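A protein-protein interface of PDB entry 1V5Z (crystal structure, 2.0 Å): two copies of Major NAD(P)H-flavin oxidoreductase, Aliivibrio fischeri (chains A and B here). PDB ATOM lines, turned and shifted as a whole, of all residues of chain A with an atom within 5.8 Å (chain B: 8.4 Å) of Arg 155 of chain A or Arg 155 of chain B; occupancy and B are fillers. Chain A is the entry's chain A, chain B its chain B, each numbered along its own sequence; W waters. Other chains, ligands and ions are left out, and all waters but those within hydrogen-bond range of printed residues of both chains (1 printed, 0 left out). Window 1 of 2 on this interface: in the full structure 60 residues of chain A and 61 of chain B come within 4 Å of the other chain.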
ATOM      1  N   PRO A   3       4.108 -21.293  32.464  1.00  0.00           N
ATOM      2  CA  PRO A   3       3.107 -20.260  32.170  1.00  0.00           C
ATOM      3  C   PRO A   3       2.530 -20.290  30.744  1.00  0.00           C
ATOM      4  O   PRO A   3       1.329 -20.163  30.576  1.00  0.00           O
ATOM      5  CB  PRO A   3       3.879 -18.950  32.440  1.00  0.00           C
ATOM      6  CG  PRO A   3       4.819 -19.321  33.502  1.00  0.00           C
ATOM      7  CD  PRO A   3       5.311 -20.696  33.076  1.00  0.00           C
ATOM      8  N   ILE A   4       3.380 -20.448  29.731  1.00  0.00           N
ATOM      9  CA  ILE A   4       2.909 -20.458  28.335  1.00  0.00           C
ATOM     10  C   ILE A   4       2.003 -21.648  28.021  1.00  0.00           C
ATOM     11  O   ILE A   4       0.923 -21.488  27.451  1.00  0.00           O
ATOM     12  CB  ILE A   4       4.080 -20.405  27.339  1.00  0.00           C
ATOM     13  CG1 ILE A   4       4.912 -19.150  27.573  1.00  0.00           C
ATOM     14  CG2 ILE A   4       3.576 -20.410  25.925  1.00  0.00           C
ATOM     15  CD1 ILE A   4       6.108 -18.979  26.651  1.00  0.00           C
ATOM     16  N   ASP A   7      -1.460 -21.341  29.722  1.00  0.00           N
ATOM     17  CA  ASP A   7      -2.352 -20.447  29.013  1.00  0.00           C
ATOM     18  C   ASP A   7      -2.995 -21.111  27.827  1.00  0.00           C
ATOM     19  O   ASP A   7      -4.208 -21.061  27.672  1.00  0.00           O
ATOM     20  CB  ASP A   7      -1.616 -19.194  28.547  1.00  0.00           C
ATOM     21  CG  ASP A   7      -1.280 -18.247  29.704  1.00  0.00           C
ATOM     22  OD1 ASP A   7      -1.793 -18.459  30.827  1.00  0.00           O
ATOM     23  OD2 ASP A   7      -0.507 -17.302  29.476  1.00  0.00           O
ATOM     24  N   LEU A 150      -5.622 -14.634  19.852  1.00  0.00           N
ATOM     25  CA  LEU A 150      -6.024 -15.753  20.688  1.00  0.00           C
ATOM     26  C   LEU A 150      -5.047 -15.985  21.834  1.00  0.00           C
ATOM     27  O   LEU A 150      -5.464 -16.288  22.951  1.00  0.00           O
ATOM     28  CB  LEU A 150      -6.203 -17.027  19.863  1.00  0.00           C
ATOM     29  CG  LEU A 150      -7.370 -17.089  18.873  1.00  0.00           C
ATOM     30  CD1 LEU A 150      -7.277 -18.400  18.088  1.00  0.00           C
ATOM     31  CD2 LEU A 150      -8.731 -16.971  19.593  1.00  0.00           C
ATOM     32  N   HIS A 151      -3.764 -15.810  21.561  1.00  0.00           N
ATOM     33  CA  HIS A 151      -2.742 -15.982  22.593  1.00  0.00           C
ATOM     34  C   HIS A 151      -2.902 -14.820  23.603  1.00  0.00           C
ATOM     35  O   HIS A 151      -2.808 -15.023  24.801  1.00  0.00           O
ATOM     36  CB  HIS A 151      -1.324 -15.980  21.975  1.00  0.00           C
ATOM     37  CG  HIS A 151      -0.254 -16.510  22.889  1.00  0.00           C
ATOM     38  ND1 HIS A 151       0.646 -17.483  22.503  1.00  0.00           N
ATOM     39  CD2 HIS A 151       0.067 -16.201  24.169  1.00  0.00           C
ATOM     40  CE1 HIS A 151       1.471 -17.752  23.503  1.00  0.00           C
ATOM     41  NE2 HIS A 151       1.140 -16.988  24.524  1.00  0.00           N
ATOM     42  N   THR A 152      -3.162 -13.618  23.095  1.00  0.00           N
ATOM     43  CA  THR A 152      -3.344 -12.426  23.929  1.00  0.00           C
ATOM     44  C   THR A 152      -4.514 -12.602  24.892  1.00  0.00           C
ATOM     45  O   THR A 152      -4.405 -12.303  26.074  1.00  0.00           O
ATOM     46  CB  THR A 152      -3.584 -11.169  23.049  1.00  0.00           C
ATOM     47  OG1 THR A 152      -2.396 -10.861  22.317  1.00  0.00           O
ATOM     48  CG2 THR A 152      -3.967  -9.951  23.905  1.00  0.00           C
ATOM     49  N   LEU A 153      -5.622 -13.118  24.388  1.00  0.00           N
ATOM     50  CA  LEU A 153      -6.811 -13.341  25.193  1.00  0.00           C
ATOM     51  C   LEU A 153      -6.608 -14.407  26.259  1.00  0.00           C
ATOM     52  O   LEU A 153      -7.188 -14.336  27.353  1.00  0.00           O
ATOM     53  CB  LEU A 153      -7.976 -13.717  24.299  1.00  0.00           C
ATOM     54  CG  LEU A 153      -8.487 -12.602  23.401  1.00  0.00           C
ATOM     55  CD1 LEU A 153      -9.389 -13.184  22.335  1.00  0.00           C
ATOM     56  CD2 LEU A 153      -9.243 -11.607  24.249  1.00  0.00           C
ATOM     57  N   ALA A 154      -5.769 -15.390  25.956  1.00  0.00           N
ATOM     58  CA  ALA A 154      -5.487 -16.444  26.921  1.00  0.00           C
ATOM     59  C   ALA A 154      -4.715 -15.811  28.081  1.00  0.00           C
ATOM     60  O   ALA A 154      -4.926 -16.166  29.241  1.00  0.00           O
ATOM     61  CB  ALA A 154      -4.659 -17.574  26.263  1.00  0.00           C
ATOM     62  N   ARG A 155      -3.855 -14.838  27.782  1.00  0.00           N
ATOM     63  CA  ARG A 155      -3.082 -14.166  28.837  1.00  0.00           C
ATOM     64  C   ARG A 155      -3.913 -13.240  29.723  1.00  0.00           C
ATOM     65  O   ARG A 155      -3.599 -13.063  30.893  1.00  0.00           O
ATOM     66  CB  ARG A 155      -1.907 -13.394  28.232  1.00  0.00           C
ATOM     67  CG  ARG A 155      -0.890 -14.309  27.530  1.00  0.00           C
ATOM     68  CD  ARG A 155       0.253 -13.528  26.964  1.00  0.00           C
ATOM     69  NE  ARG A 155       1.056 -12.938  28.028  1.00  0.00           N
ATOM     70  CZ  ARG A 155       2.169 -12.252  27.813  1.00  0.00           C
ATOM     71  NH1 ARG A 155       2.599 -12.071  26.571  1.00  0.00           N
ATOM     72  NH2 ARG A 155       2.889 -11.800  28.833  1.00  0.00           N
ATOM     73  N   LEU A 156      -4.985 -12.684  29.161  1.00  0.00           N
ATOM     74  CA  LEU A 156      -5.871 -11.753  29.873  1.00  0.00           C
ATOM     75  C   LEU A 156      -7.009 -12.474  30.566  1.00  0.00           C
ATOM     76  O   LEU A 156      -7.806 -11.847  31.270  1.00  0.00           O
ATOM     77  CB  LEU A 156      -6.455 -10.699  28.889  1.00  0.00           C
ATOM     78  CG  LEU A 156      -5.491  -9.650  28.309  1.00  0.00           C
ATOM     79  CD1 LEU A 156      -6.104  -8.952  27.126  1.00  0.00           C
ATOM     80  CD2 LEU A 156      -5.059  -8.680  29.398  1.00  0.00           C
ATOM     81  N   ASN A 157      -7.111 -13.780  30.322  1.00  0.00           N
ATOM     82  CA  ASN A 157      -8.170 -14.602  30.900  1.00  0.00           C
ATOM     83  C   ASN A 157      -9.581 -14.174  30.510  1.00  0.00           C
ATOM     84  O   ASN A 157     -10.490 -14.085  31.351  1.00  0.00           O
ATOM     85  CB  ASN A 157      -8.014 -14.687  32.413  1.00  0.00           C
ATOM     86  CG  ASN A 157      -6.894 -15.630  32.816  1.00  0.00           C
ATOM     87  OD1 ASN A 157      -7.074 -16.841  32.822  1.00  0.00           O
ATOM     88  ND2 ASN A 157      -5.738 -15.077  33.138  1.00  0.00           N
ATOM     89  N   HIS B   2       2.645  -2.774  30.590  1.00  0.00           N
ATOM     90  CA  HIS B   2       1.826  -3.978  30.715  1.00  0.00           C
ATOM     91  C   HIS B   2       2.667  -5.126  30.105  1.00  0.00           C
ATOM     92  O   HIS B   2       3.317  -4.932  29.082  1.00  0.00           O
ATOM     93  CB  HIS B   2       0.533  -3.754  29.939  1.00  0.00           C
ATOM     94  CG  HIS B   2      -0.484  -4.838  30.111  1.00  0.00           C
ATOM     95  ND1 HIS B   2      -0.315  -6.117  29.613  1.00  0.00           N
ATOM     96  CD2 HIS B   2      -1.706  -4.820  30.692  1.00  0.00           C
ATOM     97  CE1 HIS B   2      -1.389  -6.836  29.883  1.00  0.00           C
ATOM     98  NE2 HIS B   2      -2.248  -6.073  30.537  1.00  0.00           N
ATOM     99  N   PRO B   3       2.732  -6.293  30.774  1.00  0.00           N
ATOM    100  CA  PRO B   3       3.517  -7.441  30.274  1.00  0.00           C
ATOM    101  C   PRO B   3       3.247  -7.816  28.808  1.00  0.00           C
ATOM    102  O   PRO B   3       4.185  -8.024  28.060  1.00  0.00           O
ATOM    103  CB  PRO B   3       3.111  -8.567  31.214  1.00  0.00           C
ATOM    104  CG  PRO B   3       2.860  -7.845  32.485  1.00  0.00           C
ATOM    105  CD  PRO B   3       2.084  -6.640  32.050  1.00  0.00           C
ATOM    106  N   ILE B   4       1.983  -7.856  28.393  1.00  0.00           N
ATOM    107  CA  ILE B   4       1.657  -8.230  27.017  1.00  0.00           C
ATOM    108  C   ILE B   4       2.191  -7.230  25.983  1.00  0.00           C
ATOM    109  O   ILE B   4       2.855  -7.608  25.003  1.00  0.00           O
ATOM    110  CB  ILE B   4       0.139  -8.456  26.850  1.00  0.00           C
ATOM    111  CG1 ILE B   4      -0.338  -9.535  27.819  1.00  0.00           C
ATOM    112  CG2 ILE B   4      -0.181  -8.870  25.430  1.00  0.00           C
ATOM    113  CD1 ILE B   4      -1.810  -9.853  27.712  1.00  0.00           C
ATOM    114  N   ILE B   5       1.938  -5.947  26.222  1.00  0.00           N
ATOM    115  CA  ILE B   5       2.407  -4.899  25.327  1.00  0.00           C
ATOM    116  C   ILE B   5       3.933  -4.870  25.260  1.00  0.00           C
ATOM    117  O   ILE B   5       4.506  -4.666  24.196  1.00  0.00           O
ATOM    118  CB  ILE B   5       1.875  -3.527  25.777  1.00  0.00           C
ATOM    119  CG1 ILE B   5       0.351  -3.547  25.738  1.00  0.00           C
ATOM    120  CG2 ILE B   5       2.460  -2.430  24.917  1.00  0.00           C
ATOM    121  CD1 ILE B   5      -0.222  -4.021  24.385  1.00  0.00           C
ATOM    122  N   HIS B   6       4.583  -5.054  26.405  1.00  0.00           N
ATOM    123  CA  HIS B   6       6.031  -5.065  26.456  1.00  0.00           C
ATOM    124  C   HIS B   6       6.605  -6.151  25.551  1.00  0.00           C
ATOM    125  O   HIS B   6       7.569  -5.895  24.836  1.00  0.00           O
ATOM    126  CB  HIS B   6       6.513  -5.308  27.877  1.00  0.00           C
ATOM    127  CG  HIS B   6       7.998  -5.334  27.999  1.00  0.00           C
ATOM    128  ND1 HIS B   6       8.740  -4.188  28.124  1.00  0.00           N
ATOM    129  CD2 HIS B   6       8.882  -6.353  27.939  1.00  0.00           C
ATOM    130  CE1 HIS B   6      10.021  -4.493  28.131  1.00  0.00           C
ATOM    131  NE2 HIS B   6      10.136  -5.801  28.018  1.00  0.00           N
ATOM    132  N   ASP B   7       6.006  -7.343  25.592  1.00  0.00           N
ATOM    133  CA  ASP B   7       6.456  -8.473  24.773  1.00  0.00           C
ATOM    134  C   ASP B   7       6.300  -8.172  23.287  1.00  0.00           C
ATOM    135  O   ASP B   7       7.235  -8.304  22.514  1.00  0.00           O
ATOM    136  CB  ASP B   7       5.666  -9.745  25.113  1.00  0.00           C
ATOM    137  CG  ASP B   7       6.060 -10.349  26.452  1.00  0.00           C
ATOM    138  OD1 ASP B   7       7.075  -9.927  27.048  1.00  0.00           O
ATOM    139  OD2 ASP B   7       5.345 -11.258  26.915  1.00  0.00           O
ATOM    140  N   LEU B   8       5.131  -7.695  22.914  1.00  0.00           N
ATOM    141  CA  LEU B   8       4.860  -7.373  21.527  1.00  0.00           C
ATOM    142  C   LEU B   8       5.584  -6.136  20.982  1.00  0.00           C
ATOM    143  O   LEU B   8       5.753  -5.993  19.775  1.00  0.00           O
ATOM    144  CB  LEU B   8       3.358  -7.303  21.311  1.00  0.00           C
ATOM    145  CG  LEU B   8       2.645  -8.630  21.602  1.00  0.00           C
ATOM    146  CD1 LEU B   8       1.158  -8.449  21.403  1.00  0.00           C
ATOM    147  CD2 LEU B   8       3.160  -9.720  20.683  1.00  0.00           C
ATOM    148  N   ARG B  11       9.523  -7.586  20.636  1.00  0.00           N
ATOM    149  CA  ARG B  11       9.832  -8.598  19.622  1.00  0.00           C
ATOM    150  C   ARG B  11       9.984  -7.844  18.292  1.00  0.00           C
ATOM    151  O   ARG B  11       9.384  -6.782  18.106  1.00  0.00           O
ATOM    152  CB  ARG B  11       8.722  -9.659  19.522  1.00  0.00           C
ATOM    153  CG  ARG B  11       7.368  -9.159  19.041  1.00  0.00           C
ATOM    154  CD  ARG B  11       6.618 -10.195  18.180  1.00  0.00           C
ATOM    155  NE  ARG B  11       7.355 -10.520  16.955  1.00  0.00           N
ATOM    156  CZ  ARG B  11       7.515  -9.698  15.920  1.00  0.00           C
ATOM    157  NH1 ARG B  11       6.975  -8.485  15.921  1.00  0.00           N
ATOM    158  NH2 ARG B  11       8.279 -10.066  14.905  1.00  0.00           N
ATOM    159  N   ASP B  27      13.406 -24.866  25.969  1.00  0.00           N
ATOM    160  CA  ASP B  27      12.636 -23.820  25.292  1.00  0.00           C
ATOM    161  C   ASP B  27      12.038 -24.323  23.974  1.00  0.00           C
ATOM    162  O   ASP B  27      10.925 -23.932  23.605  1.00  0.00           O
ATOM    163  CB  ASP B  27      13.512 -22.603  24.983  1.00  0.00           C
ATOM    164  CG  ASP B  27      13.737 -21.687  26.184  1.00  0.00           C
ATOM    165  OD1 ASP B  27      13.062 -21.830  27.220  1.00  0.00           O
ATOM    166  OD2 ASP B  27      14.594 -20.795  26.071  1.00  0.00           O
ATOM    167  N   VAL B  30       8.804 -26.235  24.614  1.00  0.00           N
ATOM    168  CA  VAL B  30       7.680 -25.369  24.984  1.00  0.00           C
ATOM    169  C   VAL B  30       7.068 -24.779  23.714  1.00  0.00           C
ATOM    170  O   VAL B  30       5.861 -24.792  23.542  1.00  0.00           O
ATOM    171  CB  VAL B  30       8.130 -24.243  25.943  1.00  0.00           C
ATOM    172  CG1 VAL B  30       7.018 -23.193  26.105  1.00  0.00           C
ATOM    173  CG2 VAL B  30       8.506 -24.856  27.290  1.00  0.00           C
ATOM    174  N   ASN B 148       0.575 -17.494  16.594  1.00  0.00           N
ATOM    175  CA  ASN B 148       0.685 -18.062  17.923  1.00  0.00           C
ATOM    176  C   ASN B 148       2.175 -18.243  18.272  1.00  0.00           C
ATOM    177  O   ASN B 148       2.627 -17.819  19.345  1.00  0.00           O
ATOM    178  CB  ASN B 148      -0.039 -19.408  17.951  1.00  0.00           C
ATOM    179  CG  ASN B 148      -0.075 -20.018  19.327  1.00  0.00           C
ATOM    180  OD1 ASN B 148      -0.113 -19.308  20.332  1.00  0.00           O
ATOM    181  ND2 ASN B 148      -0.065 -21.343  19.385  1.00  0.00           N
ATOM    182  N   ALA B 149       2.952 -18.762  17.320  1.00  0.00           N
ATOM    183  CA  ALA B 149       4.382 -18.992  17.532  1.00  0.00           C
ATOM    184  C   ALA B 149       5.166 -17.717  17.833  1.00  0.00           C
ATOM    185  O   ALA B 149       6.076 -17.718  18.668  1.00  0.00           O
ATOM    186  CB  ALA B 149       4.996 -19.691  16.316  1.00  0.00           C
ATOM    187  N   LEU B 150       4.852 -16.651  17.105  1.00  0.00           N
ATOM    188  CA  LEU B 150       5.543 -15.372  17.283  1.00  0.00           C
ATOM    189  C   LEU B 150       5.290 -14.776  18.663  1.00  0.00           C
ATOM    190  O   LEU B 150       6.193 -14.195  19.254  1.00  0.00           O
ATOM    191  CB  LEU B 150       5.148 -14.367  16.181  1.00  0.00           C
ATOM    192  CG  LEU B 150       5.615 -14.632  14.738  1.00  0.00           C
ATOM    193  CD1 LEU B 150       5.005 -13.573  13.802  1.00  0.00           C
ATOM    194  CD2 LEU B 150       7.148 -14.653  14.643  1.00  0.00           C
ATOM    195  N   HIS B 151       4.066 -14.911  19.162  1.00  0.00           N
ATOM    196  CA  HIS B 151       3.727 -14.409  20.491  1.00  0.00           C
ATOM    197  C   HIS B 151       4.473 -15.279  21.521  1.00  0.00           C
ATOM    198  O   HIS B 151       5.047 -14.756  22.468  1.00  0.00           O
ATOM    199  CB  HIS B 151       2.206 -14.473  20.723  1.00  0.00           C
ATOM    200  CG  HIS B 151       1.735 -13.664  21.910  1.00  0.00           C
ATOM    201  ND1 HIS B 151       0.709 -12.742  21.828  1.00  0.00           N
ATOM    202  CD2 HIS B 151       2.148 -13.645  23.201  1.00  0.00           C
ATOM    203  CE1 HIS B 151       0.513 -12.191  23.015  1.00  0.00           C
ATOM    204  NE2 HIS B 151       1.371 -12.720  23.865  1.00  0.00           N
ATOM    205  N   THR B 152       4.512 -16.594  21.286  1.00  0.00           N
ATOM    206  CA  THR B 152       5.197 -17.537  22.158  1.00  0.00           C
ATOM    207  C   THR B 152       6.690 -17.202  22.259  1.00  0.00           C
ATOM    208  O   THR B 152       7.266 -17.205  23.348  1.00  0.00           O
ATOM    209  CB  THR B 152       5.020 -18.983  21.627  1.00  0.00           C
ATOM    210  OG1 THR B 152       3.645 -19.360  21.710  1.00  0.00           O
ATOM    211  CG2 THR B 152       5.869 -19.979  22.427  1.00  0.00           C
ATOM    212  N   LEU B 153       7.311 -16.896  21.126  1.00  0.00           N
ATOM    213  CA  LEU B 153       8.733 -16.565  21.091  1.00  0.00           C
ATOM    214  C   LEU B 153       9.044 -15.256  21.810  1.00  0.00           C
ATOM    215  O   LEU B 153      10.107 -15.084  22.417  1.00  0.00           O
ATOM    216  CB  LEU B 153       9.224 -16.509  19.644  1.00  0.00           C
ATOM    217  CG  LEU B 153       9.286 -17.875  18.949  1.00  0.00           C
ATOM    218  CD1 LEU B 153       9.490 -17.672  17.464  1.00  0.00           C
ATOM    219  CD2 LEU B 153      10.418 -18.713  19.551  1.00  0.00           C
ATOM    220  N   ALA B 154       8.106 -14.330  21.755  1.00  0.00           N
ATOM    221  CA  ALA B 154       8.299 -13.054  22.434  1.00  0.00           C
ATOM    222  C   ALA B 154       8.310 -13.310  23.945  1.00  0.00           C
ATOM    223  O   ALA B 154       9.097 -12.722  24.652  1.00  0.00           O
ATOM    224  CB  ALA B 154       7.198 -12.083  22.059  1.00  0.00           C
ATOM    225  N   ARG B 155       7.494 -14.249  24.420  1.00  0.00           N
ATOM    226  CA  ARG B 155       7.447 -14.595  25.841  1.00  0.00           C
ATOM    227  C   ARG B 155       8.688 -15.334  26.326  1.00  0.00           C
ATOM    228  O   ARG B 155       9.059 -15.218  27.497  1.00  0.00           O
ATOM    229  CB  ARG B 155       6.192 -15.422  26.162  1.00  0.00           C
ATOM    230  CG  ARG B 155       4.898 -14.664  25.884  1.00  0.00           C
ATOM    231  CD  ARG B 155       3.684 -15.458  26.236  1.00  0.00           C
ATOM    232  NE  ARG B 155       3.590 -15.682  27.669  1.00  0.00           N
ATOM    233  CZ  ARG B 155       2.574 -16.302  28.249  1.00  0.00           C
ATOM    234  NH1 ARG B 155       1.580 -16.757  27.505  1.00  0.00           N
ATOM    235  NH2 ARG B 155       2.529 -16.449  29.566  1.00  0.00           N
ATOM    236  N   LEU B 156       9.324 -16.098  25.430  1.00  0.00           N
ATOM    237  CA  LEU B 156      10.526 -16.878  25.770  1.00  0.00           C
ATOM    238  C   LEU B 156      11.813 -16.092  25.573  1.00  0.00           C
ATOM    239  O   LEU B 156      12.897 -16.547  25.958  1.00  0.00           O
ATOM    240  CB  LEU B 156      10.567 -18.176  24.938  1.00  0.00           C
ATOM    241  CG  LEU B 156       9.536 -19.261  25.269  1.00  0.00           C
ATOM    242  CD1 LEU B 156       9.488 -20.294  24.160  1.00  0.00           C
ATOM    243  CD2 LEU B 156       9.837 -19.892  26.627  1.00  0.00           C
ATOM    244  N   ASN B 157      11.689 -14.909  24.969  1.00  0.00           N
ATOM    245  CA  ASN B 157      12.822 -14.033  24.697  1.00  0.00           C
ATOM    246  C   ASN B 157      13.837 -14.638  23.729  1.00  0.00           C
ATOM    247  O   ASN B 157      15.063 -14.579  23.947  1.00  0.00           O
ATOM    248  CB  ASN B 157      13.479 -13.573  26.006  1.00  0.00           C
ATOM    249  CG  ASN B 157      12.666 -12.482  26.700  1.00  0.00           C
ATOM    250  OD1 ASN B 157      12.692 -11.321  26.292  1.00  0.00           O
ATOM    251  ND2 ASN B 157      11.934 -12.856  27.733  1.00  0.00           N
ATOM    252  N   ILE B 158      13.299 -15.240  22.669  1.00  0.00           N
ATOM    253  CA  ILE B 158      14.095 -15.862  21.618  1.00  0.00           C
ATOM    254  C   ILE B 158      13.865 -15.030  20.369  1.00  0.00           C
ATOM    255  O   ILE B 158      12.733 -14.666  20.090  1.00  0.00           O
ATOM    256  CB  ILE B 158      13.606 -17.311  21.338  1.00  0.00           C
ATOM    257  CG1 ILE B 158      13.856 -18.203  22.562  1.00  0.00           C
ATOM    258  CG2 ILE B 158      14.324 -17.884  20.152  1.00  0.00           C
ATOM    259  CD1 ILE B 158      13.299 -19.624  22.422  1.00  0.00           C
HETATM  260  O   HOH W   1      -3.063 -18.588  19.593  1.00  0.00           O
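A ring nitrogen (NE2) of His 151 of chain A is in hydrogen-bond range of the guanidinium group of Arg 155 of chain B, 3.0 Å away.
The side-chain carboxylate of Asp 7 of chain A is in salt-bridge range of the guanidinium group of Arg 155 of chain B, at 2.9 Å.
NE2 of His 151 of chain B lies within hydrogen-bond range of NH1 of Arg 155 of chain A, at 3.0 Å.
A ring nitrogen (ND1) of His 151 of chain A sits at hydrogen-bond distance from the side-chain amide oxygen of Asn 148 of chain B.
The guanidinium group of Arg 155 of chain A lies within salt-bridge range of the side-chain carboxylate of Asp 7 of chain B (2.9 Å).
O of Asn 148 of chain B is in hydrogen-bond range of OG1 of Thr 152 of chain B (3.0 Å).
ND1 of His 2 of chain B lies within hydrogen-bond range of N of Ile 4 of chain B, at 3.1 Å.
Among the printed residues, merely in contact across the chains: Ile 4 of chain A with Thr 152 of chain B (3.9 Å), Ile 4 of chain A with Arg 155 of chain B (3.6 Å), Ile 4 of chain A with Leu 156 of chain B (3.7 Å), His 151 of chain A with His 151 of chain B (3.4 Å), His 151 of chain A with Thr 152 of chain B (3.2 Å), Thr 152 of chain A with Ile 4 of chain B (3.9 Å), Thr 152 of chain A with His 151 of chain B (3.3 Å), Arg 155 of chain A with Ile 4 of chain B (3.6 Å), Arg 155 of chain A with Arg 155 of chain B (3.5 Å), Leu 156 of chain A with His 2 of chain B (3.999 Å) and Leu 156 of chain A with Ile 4 of chain B (3.7 Å).
No residue of chain B comes within 4 Å of Ala 154 of chain A.
Of the printed residues of chain B, Arg 155 of chain A touches Ile 4, Asp 7, His 151 and Arg 155.
Printed residues of chain A within 4 Å of His 151 of chain B: His 151, Thr 152 and Arg 155.
Of the printed residues of chain A, Thr 152 of chain B touches Ile 4 (3.9 Å) and His 151 (3.2 Å).
The nearest printed residue of chain A that does not touch Arg 155 of chain B is Pro 3 of chain A (4.02 Å).
The nearest printed residue of chain A that does not touch His 2 of chain B is Arg 155 of chain A (6.6 Å).
Printed residues of chain B that touch a printed residue of chain A: His 2, Ile 4, Asp 7, Asn 148, His 151, Thr 152, Arg 155 and Leu 156.
Hydrophobic or aromatic side chains of chain B within 4 Å of the printed part of chain A: His 2, Ile 4, His 151 and Leu 156.
Of the 11 printed residues of chain A, 6 touch a printed residue of chain B.
Printed residues of chain A that touch a printed residue of chain B: Ile 4, Asp 7, His 151, Thr 152, Arg 155 and Leu 156.
Hydrophobic or aromatic side chains of chain A that line the printed part of chain B: Ile 4, His 151 and Leu 156.
Among the printed residues, Asp or Glu carboxylates within 4 Å of a Lys or Arg side-chain nitrogen of the other chain: Asp 7 of chain A with Arg 155 of chain B and Arg 155 of chain A with Asp 7 of chain B.
Ile 4 of chain A touches Thr 152 of chain B, and with the chains exchanged Thr 152 of chain A touches Ile 4 of chain B.
Ile 4 of chain A touches Arg 155 of chain B, and with the chains exchanged Arg 155 of chain A touches Ile 4 of chain B.
His 151 of chain A touches Thr 152 of chain B, and with the chains exchanged Thr 152 of chain A touches His 151 of chain B.
His 151 of chain A touches Arg 155 of chain B, and with the chains exchanged Arg 155 of chain A touches His 151 of chain B.
Positions printed for both chains: 3, 4, 7, 150, 151, 152, 153, 154, 155, 156 and 157.
Of the 16 pairs that touch across the chains among the printed residues, 14 have their exchanged pair printed and touching as well.
Water W1 bridges OD1 of Asn 148 of chain B (3.1 Å) and N of His 151 of chain A (3.5 Å).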
